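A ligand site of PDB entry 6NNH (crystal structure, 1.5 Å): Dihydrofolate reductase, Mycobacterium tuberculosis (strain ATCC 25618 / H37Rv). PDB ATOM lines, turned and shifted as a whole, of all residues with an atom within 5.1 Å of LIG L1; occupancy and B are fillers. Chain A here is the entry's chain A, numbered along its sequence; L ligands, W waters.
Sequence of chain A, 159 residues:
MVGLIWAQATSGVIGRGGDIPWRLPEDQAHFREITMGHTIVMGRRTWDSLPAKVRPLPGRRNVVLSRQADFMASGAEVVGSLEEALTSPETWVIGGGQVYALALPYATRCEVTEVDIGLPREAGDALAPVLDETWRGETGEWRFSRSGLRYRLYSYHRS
Water W1 lies within hydrogen-bond range of the side-chain hydroxyl (OG1) of Thr 113 (2.8 Å), a nitrogen (N4) of LIG L1 (2.9 Å), the backbone carbonyl oxygen (O) of Glu 111 (3.0 Å), a ring nitrogen (NE2) of His 30 (3.0 Å) and the backbone carbonyl oxygen (O) of Trp 6 (3.3 Å).
The side-chain carboxylate (OD1) of Asp 27 is in hydrogen-bond range of a nitrogen (N4) of LIG L1 (2.8 Å).
The backbone carbonyl oxygen (O) of Ile 94 lies within hydrogen-bond range of a nitrogen (N5) of LIG L1, at 2.9 Å.
The backbone carbonyl oxygen (O) of Ile 5 sits at hydrogen-bond distance from a nitrogen (N5) of LIG L1 (3.0 Å).
The backbone NH of Trp 6 lies close to a nitrogen (N2) of LIG L1 (3.5 Å).
N4 of LIG L1 lies within hydrogen-bond range of O of Trp 6 (3.3 Å).
An oxygen (O2) of LG2 L2 is in hydrogen-bond range of the backbone NH (N) of Thr 46 (3.3 Å).
The side-chain hydroxyl (OG1) of Thr 46 sits at hydrogen-bond distance from an oxygen (O2) of LG2 L2 (2.6 Å).
The backbone NH of Ala 7 is in hydrogen-bond range of an oxygen (O14) of LG2 L2.
O of Ala 7 lies within hydrogen-bond range of N7 of LG2 L2, at 2.9 Å.
The side-chain carboxylate (OD1) of Asp 27 sits at hydrogen-bond distance from the side-chain hydroxyl (OG1) of Thr 113 (2.7 Å).
The side-chain hydroxyl (OH) of Tyr 100 sits at hydrogen-bond distance from the backbone carbonyl oxygen (O) of Ile 94 (3.1 Å).
The backbone carbonyl oxygen of Ile 5 is in hydrogen-bond range of the side-chain hydroxyl of Tyr 100 (2.6 Å).
O of Trp 6 is in hydrogen-bond range of N of Thr 113 (3.0 Å).
O of Glu 111 lies within hydrogen-bond range of N of Trp 6, 3.2 Å away.
O of Thr 46 is in hydrogen-bond range of OG of Ser 49 (2.7 Å).
N of Gly 95 sits at hydrogen-bond distance from OH of Tyr 100 (3.2 Å).
Ala 7 touches LIG L1 (N to N4, 3.6 Å).
CD1 of Ile 20 touches C7 of LIG L1 (3.9 Å).
CZ of Phe 31 touches C11 of LIG L1, 3.5 Å away.
Thr 46 touches LIG L1.
CD2 of Leu 50 touches CL1 of LIG L1 (3.5 Å).
Tyr 100 touches LIG L1 (OH to N5, 3.7 Å).
Thr 113 touches LIG L1 (OG1 to N4, 3.6 Å).
Hydrophobic or aromatic side chains within 4 Å of LIG L1: Ile 5, Ala 7, Ile 20, Phe 31, Leu 50 and Ile 94.
11 residues have an atom within 4 Å of LIG L1: Ile 5, Trp 6, Ala 7, Ile 20, Asp 27, Phe 31, Thr 46, Leu 50, Ile 94, Tyr 100 and Thr 113.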
ATOM      1  N   ILE A   5     -12.773 -20.677 -12.469  1.00  0.00           N
ATOM      2  CA  ILE A   5     -12.022 -19.539 -11.949  1.00  0.00           C
ATOM      3  C   ILE A   5     -12.709 -18.267 -12.430  1.00  0.00           C
ATOM      4  O   ILE A   5     -12.988 -18.122 -13.630  1.00  0.00           O
ATOM      5  CB  ILE A   5     -10.534 -19.608 -12.376  1.00  0.00           C
ATOM      6  CG1 ILE A   5      -9.748 -18.422 -11.826  1.00  0.00           C
ATOM      7  CG2 ILE A   5     -10.368 -19.741 -13.900  1.00  0.00           C
ATOM      8  CD1 ILE A   5      -8.227 -18.645 -11.809  1.00  0.00           C
ATOM      9  N   TRP A   6     -13.010 -17.376 -11.487  1.00  0.00           N
ATOM     10  CA  TRP A   6     -13.694 -16.126 -11.804  1.00  0.00           C
ATOM     11  C   TRP A   6     -13.335 -15.086 -10.767  1.00  0.00           C
ATOM     12  O   TRP A   6     -12.848 -15.388  -9.671  1.00  0.00           O
ATOM     13  CB  TRP A   6     -15.219 -16.303 -11.879  1.00  0.00           C
ATOM     14  CG  TRP A   6     -15.953 -16.472 -10.565  1.00  0.00           C
ATOM     15  CD1 TRP A   6     -16.340 -15.488  -9.695  1.00  0.00           C
ATOM     16  CD2 TRP A   6     -16.426 -17.714  -9.997  1.00  0.00           C
ATOM     17  NE1 TRP A   6     -17.020 -16.043  -8.629  1.00  0.00           N
ATOM     18  CE2 TRP A   6     -17.095 -17.403  -8.803  1.00  0.00           C
ATOM     19  CE3 TRP A   6     -16.359 -19.055 -10.410  1.00  0.00           C
ATOM     20  CZ2 TRP A   6     -17.666 -18.383  -7.984  1.00  0.00           C
ATOM     21  CZ3 TRP A   6     -16.938 -20.031  -9.596  1.00  0.00           C
ATOM     22  CH2 TRP A   6     -17.580 -19.688  -8.395  1.00  0.00           C
ATOM     23  N   ALA A   7     -13.590 -13.817 -11.135  1.00  0.00           N
ATOM     24  CA  ALA A   7     -13.537 -12.703 -10.208  1.00  0.00           C
ATOM     25  C   ALA A   7     -14.925 -12.091 -10.135  1.00  0.00           C
ATOM     26  O   ALA A   7     -15.583 -11.919 -11.153  1.00  0.00           O
ATOM     27  CB  ALA A   7     -12.500 -11.658 -10.650  1.00  0.00           C
ATOM     28  N   ILE A  20     -16.118  -6.415 -18.255  1.00  0.00           N
ATOM     29  CA  ILE A  20     -15.945  -6.508 -16.812  1.00  0.00           C
ATOM     30  C   ILE A  20     -15.729  -5.107 -16.259  1.00  0.00           C
ATOM     31  O   ILE A  20     -14.921  -4.366 -16.811  1.00  0.00           O
ATOM     32  CB  ILE A  20     -14.752  -7.404 -16.439  1.00  0.00           C
ATOM     33  CG1 ILE A  20     -14.916  -8.758 -17.100  1.00  0.00           C
ATOM     34  CG2 ILE A  20     -14.640  -7.571 -14.921  1.00  0.00           C
ATOM     35  CD1 ILE A  20     -13.713  -9.673 -16.888  1.00  0.00           C
ATOM     36  N   ASP A  27      -5.115  -9.879  -9.914  1.00  0.00           N
ATOM     37  CA  ASP A  27      -6.051 -10.944 -10.234  1.00  0.00           C
ATOM     38  C   ASP A  27      -5.752 -11.504 -11.619  1.00  0.00           C
ATOM     39  O   ASP A  27      -5.785 -12.727 -11.822  1.00  0.00           O
ATOM     40  CB  ASP A  27      -7.467 -10.397 -10.173  1.00  0.00           C
ATOM     41  CG  ASP A  27      -8.478 -11.376 -10.717  1.00  0.00           C
ATOM     42  OD1 ASP A  27      -8.603 -12.461 -10.132  1.00  0.00           O
ATOM     43  OD2 ASP A  27      -9.126 -11.030 -11.721  1.00  0.00           O
ATOM     44  N   GLN A  28      -5.391 -10.645 -12.563  1.00  0.00           N
ATOM     45  CA  GLN A  28      -5.014 -11.137 -13.888  1.00  0.00           C
ATOM     46  C   GLN A  28      -3.806 -12.048 -13.788  1.00  0.00           C
ATOM     47  O   GLN A  28      -3.765 -13.103 -14.430  1.00  0.00           O
ATOM     48  CB  GLN A  28      -4.725  -9.959 -14.830  1.00  0.00           C
ATOM     49  CG  GLN A  28      -5.930  -9.125 -15.175  1.00  0.00           C
ATOM     50  CD  GLN A  28      -5.591  -7.996 -16.117  1.00  0.00           C
ATOM     51  OE1 GLN A  28      -4.845  -7.082 -15.770  1.00  0.00           O
ATOM     52  NE2 GLN A  28      -6.138  -8.039 -17.321  1.00  0.00           N
ATOM     53  N   HIS A  30      -2.837 -13.805 -11.119  1.00  0.00           N
ATOM     54  CA  HIS A  30      -3.308 -15.019 -10.464  1.00  0.00           C
ATOM     55  C   HIS A  30      -4.033 -15.928 -11.459  1.00  0.00           C
ATOM     56  O   HIS A  30      -3.778 -17.139 -11.511  1.00  0.00           O
ATOM     57  CB  HIS A  30      -4.195 -14.616  -9.295  1.00  0.00           C
ATOM     58  CG  HIS A  30      -5.125 -15.684  -8.818  1.00  0.00           C
ATOM     59  ND1 HIS A  30      -4.700 -16.747  -8.055  1.00  0.00           N
ATOM     60  CD2 HIS A  30      -6.462 -15.831  -8.964  1.00  0.00           C
ATOM     61  CE1 HIS A  30      -5.739 -17.512  -7.760  1.00  0.00           C
ATOM     62  NE2 HIS A  30      -6.815 -16.971  -8.289  1.00  0.00           N
ATOM     63  N   PHE A  31      -4.905 -15.341 -12.281  1.00  0.00           N
ATOM     64  CA  PHE A  31      -5.600 -16.107 -13.302  1.00  0.00           C
ATOM     65  C   PHE A  31      -4.614 -16.754 -14.259  1.00  0.00           C
ATOM     66  O   PHE A  31      -4.757 -17.934 -14.605  1.00  0.00           O
ATOM     67  CB  PHE A  31      -6.570 -15.202 -14.077  1.00  0.00           C
ATOM     68  CG  PHE A  31      -7.100 -15.837 -15.336  1.00  0.00           C
ATOM     69  CD1 PHE A  31      -8.184 -16.710 -15.303  1.00  0.00           C
ATOM     70  CD2 PHE A  31      -6.477 -15.604 -16.559  1.00  0.00           C
ATOM     71  CE1 PHE A  31      -8.632 -17.326 -16.446  1.00  0.00           C
ATOM     72  CE2 PHE A  31      -6.929 -16.229 -17.725  1.00  0.00           C
ATOM     73  CZ  PHE A  31      -8.001 -17.099 -17.664  1.00  0.00           C
ATOM     74  N   THR A  46     -17.430 -14.713 -24.101  1.00  0.00           N
ATOM     75  CA  THR A  46     -16.175 -14.385 -23.442  1.00  0.00           C
ATOM     76  C   THR A  46     -15.011 -14.389 -24.428  1.00  0.00           C
ATOM     77  O   THR A  46     -14.128 -13.518 -24.368  1.00  0.00           O
ATOM     78  CB  THR A  46     -15.959 -15.363 -22.278  1.00  0.00           C
ATOM     79  OG1 THR A  46     -16.987 -15.124 -21.304  1.00  0.00           O
ATOM     80  CG2 THR A  46     -14.585 -15.185 -21.631  1.00  0.00           C
ATOM     81  N   SER A  49     -15.045 -11.132 -26.104  1.00  0.00           N
ATOM     82  CA  SER A  49     -14.551 -10.036 -25.283  1.00  0.00           C
ATOM     83  C   SER A  49     -13.027  -9.861 -25.356  1.00  0.00           C
ATOM     84  O   SER A  49     -12.520  -8.804 -24.975  1.00  0.00           O
ATOM     85  CB  SER A  49     -15.018 -10.216 -23.823  1.00  0.00           C
ATOM     86  OG  SER A  49     -14.179 -11.128 -23.135  1.00  0.00           O
ATOM     87  N   LEU A  50     -12.292 -10.869 -25.799  1.00  0.00           N
ATOM     88  CA  LEU A  50     -10.844 -10.765 -25.918  1.00  0.00           C
ATOM     89  C   LEU A  50     -10.473 -10.082 -27.231  1.00  0.00           C
ATOM     90  O   LEU A  50     -10.935 -10.515 -28.292  1.00  0.00           O
ATOM     91  CB  LEU A  50     -10.188 -12.132 -25.875  1.00  0.00           C
ATOM     92  CG  LEU A  50     -10.196 -12.912 -24.567  1.00  0.00           C
ATOM     93  CD1 LEU A  50      -9.882 -14.364 -24.870  1.00  0.00           C
ATOM     94  CD2 LEU A  50      -9.194 -12.314 -23.565  1.00  0.00           C
ATOM     95  N   LEU A  57      -5.196 -17.168 -25.659  1.00  0.00           N
ATOM     96  CA  LEU A  57      -4.367 -16.896 -24.497  1.00  0.00           C
ATOM     97  C   LEU A  57      -3.186 -17.855 -24.502  1.00  0.00           C
ATOM     98  O   LEU A  57      -3.375 -19.066 -24.672  1.00  0.00           O
ATOM     99  CB  LEU A  57      -5.180 -17.023 -23.208  1.00  0.00           C
ATOM    100  CG  LEU A  57      -6.365 -16.067 -23.113  1.00  0.00           C
ATOM    101  CD1 LEU A  57      -6.991 -16.138 -21.720  1.00  0.00           C
ATOM    102  CD2 LEU A  57      -5.937 -14.635 -23.436  1.00  0.00           C
ATOM    103  N   ILE A  94     -13.254 -20.700 -17.602  1.00  0.00           N
ATOM    104  CA  ILE A  94     -12.860 -19.331 -17.306  1.00  0.00           C
ATOM    105  C   ILE A  94     -13.992 -18.338 -17.544  1.00  0.00           C
ATOM    106  O   ILE A  94     -13.760 -17.120 -17.502  1.00  0.00           O
ATOM    107  CB  ILE A  94     -11.588 -18.940 -18.090  1.00  0.00           C
ATOM    108  CG1 ILE A  94     -11.866 -18.869 -19.592  1.00  0.00           C
ATOM    109  CG2 ILE A  94     -10.493 -19.983 -17.838  1.00  0.00           C
ATOM    110  CD1 ILE A  94     -10.837 -17.973 -20.326  1.00  0.00           C
ATOM    111  N   GLY A  95     -15.222 -18.828 -17.773  1.00  0.00           N
ATOM    112  CA  GLY A  95     -16.418 -18.002 -17.885  1.00  0.00           C
ATOM    113  C   GLY A  95     -17.032 -18.057 -19.268  1.00  0.00           C
ATOM    114  O   GLY A  95     -16.523 -18.719 -20.176  1.00  0.00           O
ATOM    115  N   TYR A 100     -20.333 -21.113 -16.600  1.00  0.00           N
ATOM    116  CA  TYR A 100     -20.192 -21.602 -15.230  1.00  0.00           C
ATOM    117  C   TYR A 100     -21.381 -22.454 -14.811  1.00  0.00           C
ATOM    118  O   TYR A 100     -21.207 -23.472 -14.147  1.00  0.00           O
ATOM    119  CB  TYR A 100     -20.023 -20.462 -14.217  1.00  0.00           C
ATOM    120  CG  TYR A 100     -18.728 -19.692 -14.351  1.00  0.00           C
ATOM    121  CD1 TYR A 100     -17.508 -20.337 -14.479  1.00  0.00           C
ATOM    122  CD2 TYR A 100     -18.745 -18.295 -14.377  1.00  0.00           C
ATOM    123  CE1 TYR A 100     -16.325 -19.609 -14.638  1.00  0.00           C
ATOM    124  CE2 TYR A 100     -17.587 -17.566 -14.538  1.00  0.00           C
ATOM    125  CZ  TYR A 100     -16.372 -18.221 -14.643  1.00  0.00           C
ATOM    126  OH  TYR A 100     -15.237 -17.500 -14.836  1.00  0.00           O
ATOM    127  N   GLU A 111     -11.760 -21.235  -7.908  1.00  0.00           N
ATOM    128  CA  GLU A 111     -10.784 -20.241  -7.486  1.00  0.00           C
ATOM    129  C   GLU A 111     -11.453 -18.880  -7.704  1.00  0.00           C
ATOM    130  O   GLU A 111     -11.627 -18.443  -8.853  1.00  0.00           O
ATOM    131  CB  GLU A 111      -9.480 -20.374  -8.264  1.00  0.00           C
ATOM    132  CG  GLU A 111      -8.683 -21.617  -7.915  1.00  0.00           C
ATOM    133  CD  GLU A 111      -8.140 -21.551  -6.491  1.00  0.00           C
ATOM    134  OE1 GLU A 111      -7.787 -20.439  -6.061  1.00  0.00           O
ATOM    135  OE2 GLU A 111      -8.107 -22.598  -5.812  1.00  0.00           O
ATOM    136  N   THR A 113     -11.888 -14.777  -6.946  1.00  0.00           N
ATOM    137  CA  THR A 113     -11.394 -13.505  -6.456  1.00  0.00           C
ATOM    138  C   THR A 113     -12.608 -12.660  -6.115  1.00  0.00           C
ATOM    139  O   THR A 113     -13.438 -12.385  -6.991  1.00  0.00           O
ATOM    140  CB  THR A 113     -10.553 -12.786  -7.509  1.00  0.00           C
ATOM    141  OG1 THR A 113      -9.460 -13.634  -7.886  1.00  0.00           O
ATOM    142  CG2 THR A 113     -10.014 -11.462  -6.960  1.00  0.00           C
HETATM  143  N1  LIG L   1      -9.878 -13.064 -13.310  1.00  0.00           N
HETATM  144  C1  LIG L   1     -10.303 -14.278 -12.667  1.00  0.00           C
HETATM  145  N2  LIG L   1     -10.960 -15.294 -13.403  1.00  0.00           N
HETATM  146  C2  LIG L   1     -11.199 -15.092 -14.786  1.00  0.00           C
HETATM  147  N3  LIG L   1     -10.811 -13.892 -15.445  1.00  0.00           N
HETATM  148  C3  LIG L   1     -10.192 -12.812 -14.696  1.00  0.00           C
HETATM  149  N4  LIG L   1     -10.062 -14.515 -11.297  1.00  0.00           N
HETATM  150  N5  LIG L   1     -11.845 -16.115 -15.504  1.00  0.00           N
HETATM  151  C4  LIG L   1      -8.948 -12.266 -15.378  1.00  0.00           C
HETATM  152  C5  LIG L   1     -11.295 -11.764 -14.568  1.00  0.00           C
HETATM  153  C6  LIG L   1     -11.063 -13.794 -16.860  1.00  0.00           C
HETATM  154  C7  LIG L   1     -12.212 -13.250 -17.369  1.00  0.00           C
HETATM  155  C8  LIG L   1     -12.346 -13.204 -18.749  1.00  0.00           C
HETATM  156  C9  LIG L   1     -11.342 -13.711 -19.544  1.00  0.00           C
HETATM  157  C10 LIG L   1     -10.184 -14.259 -19.030  1.00  0.00           C
HETATM  158  C11 LIG L   1     -10.051 -14.316 -17.660  1.00  0.00           C
HETATM  159 CL1  LIG L   1     -11.523 -13.642 -21.292  1.00  0.00          CL
HETATM  160  P1  LG2 L   2     -20.701 -16.780 -21.865  1.00  0.00           P
HETATM  161  O1  LG2 L   2     -21.182 -17.740 -20.835  1.00  0.00           O
HETATM  162  O2  LG2 L   2     -19.284 -16.304 -21.892  1.00  0.00           O
HETATM  163  O3  LG2 L   2     -20.968 -17.322 -23.387  1.00  0.00           O
HETATM  164  C1  LG2 L   2     -22.378 -17.616 -23.631  1.00  0.00           C
HETATM  165  C2  LG2 L   2     -22.373 -18.341 -25.003  1.00  0.00           C
HETATM  166  O4  LG2 L   2     -21.918 -19.669 -24.807  1.00  0.00           O
HETATM  167  C3  LG2 L   2     -23.765 -18.451 -25.684  1.00  0.00           C
HETATM  168  O5  LG2 L   2     -24.068 -17.274 -26.398  1.00  0.00           O
HETATM  169  C4  LG2 L   2     -23.461 -19.600 -26.676  1.00  0.00           C
HETATM  170  O6  LG2 L   2     -22.649 -19.253 -27.658  1.00  0.00           O
HETATM  171  C5  LG2 L   2     -22.602 -20.525 -25.736  1.00  0.00           C
HETATM  172  N1  LG2 L   2     -23.465 -21.383 -25.007  1.00  0.00           N
HETATM  173  C6  LG2 L   2     -24.260 -21.126 -23.888  1.00  0.00           C
HETATM  174  N2  LG2 L   2     -24.970 -22.212 -23.513  1.00  0.00           N
HETATM  175  C7  LG2 L   2     -24.624 -23.182 -24.452  1.00  0.00           C
HETATM  176  C8  LG2 L   2     -25.021 -24.512 -24.622  1.00  0.00           C
HETATM  177  N3  LG2 L   2     -25.927 -25.085 -23.756  1.00  0.00           N
HETATM  178  N4  LG2 L   2     -24.504 -25.262 -25.645  1.00  0.00           N
HETATM  179  C9  LG2 L   2     -23.609 -24.629 -26.461  1.00  0.00           C
HETATM  180  N5  LG2 L   2     -23.149 -23.370 -26.416  1.00  0.00           N
HETATM  181  C10 LG2 L   2     -23.686 -22.678 -25.392  1.00  0.00           C
HETATM  182  O7  LG2 L   2     -21.745 -15.462 -21.886  1.00  0.00           O
HETATM  183  P2  LG2 L   2     -22.179 -14.682 -20.568  1.00  0.00           P
HETATM  184  O8  LG2 L   2     -22.851 -13.491 -21.150  1.00  0.00           O
HETATM  185  O9  LG2 L   2     -22.870 -15.511 -19.521  1.00  0.00           O
HETATM  186  O10 LG2 L   2     -20.736 -14.166 -19.750  1.00  0.00           O
HETATM  187  C11 LG2 L   2     -20.065 -13.153 -20.470  1.00  0.00           C
HETATM  188  C12 LG2 L   2     -19.849 -12.002 -19.503  1.00  0.00           C
HETATM  189  O11 LG2 L   2     -19.065 -12.460 -18.376  1.00  0.00           O
HETATM  190  C13 LG2 L   2     -19.043 -10.860 -20.136  1.00  0.00           C
HETATM  191  O12 LG2 L   2     -19.473  -9.672 -19.498  1.00  0.00           O
HETATM  192  C14 LG2 L   2     -17.613 -11.207 -19.697  1.00  0.00           C
HETATM  193  O13 LG2 L   2     -16.782 -10.059 -19.684  1.00  0.00           O
HETATM  194  C15 LG2 L   2     -17.886 -11.666 -18.256  1.00  0.00           C
HETATM  195  N6  LG2 L   2     -16.798 -12.552 -17.720  1.00  0.00           N
HETATM  196  C16 LG2 L   2     -16.280 -12.271 -16.465  1.00  0.00           C
HETATM  197  C17 LG2 L   2     -15.497 -13.174 -15.827  1.00  0.00           C
HETATM  198  C18 LG2 L   2     -14.958 -12.850 -14.524  1.00  0.00           C
HETATM  199  O14 LG2 L   2     -14.282 -13.652 -13.893  1.00  0.00           O
HETATM  200  N7  LG2 L   2     -15.187 -11.591 -13.982  1.00  0.00           N
HETATM  201  C19 LG2 L   2     -15.181 -14.522 -16.400  1.00  0.00           C
HETATM  202  C20 LG2 L   2     -15.547 -14.588 -17.861  1.00  0.00           C
HETATM  203  C21 LG2 L   2     -16.310 -13.652 -18.461  1.00  0.00           C
HETATM  204  P3  LG2 L   2     -23.387 -18.895 -29.229  1.00  0.00           P
HETATM  205  O15 LG2 L   2     -24.153 -17.652 -28.882  1.00  0.00           O
HETATM  206  O16 LG2 L   2     -22.169 -18.684 -30.130  1.00  0.00           O
HETATM  207  O17 LG2 L   2     -24.182 -20.151 -29.442  1.00  0.00           O
HETATM  208  O   HOH W   1      -9.680 -16.229  -8.986  1.00  0.00           O
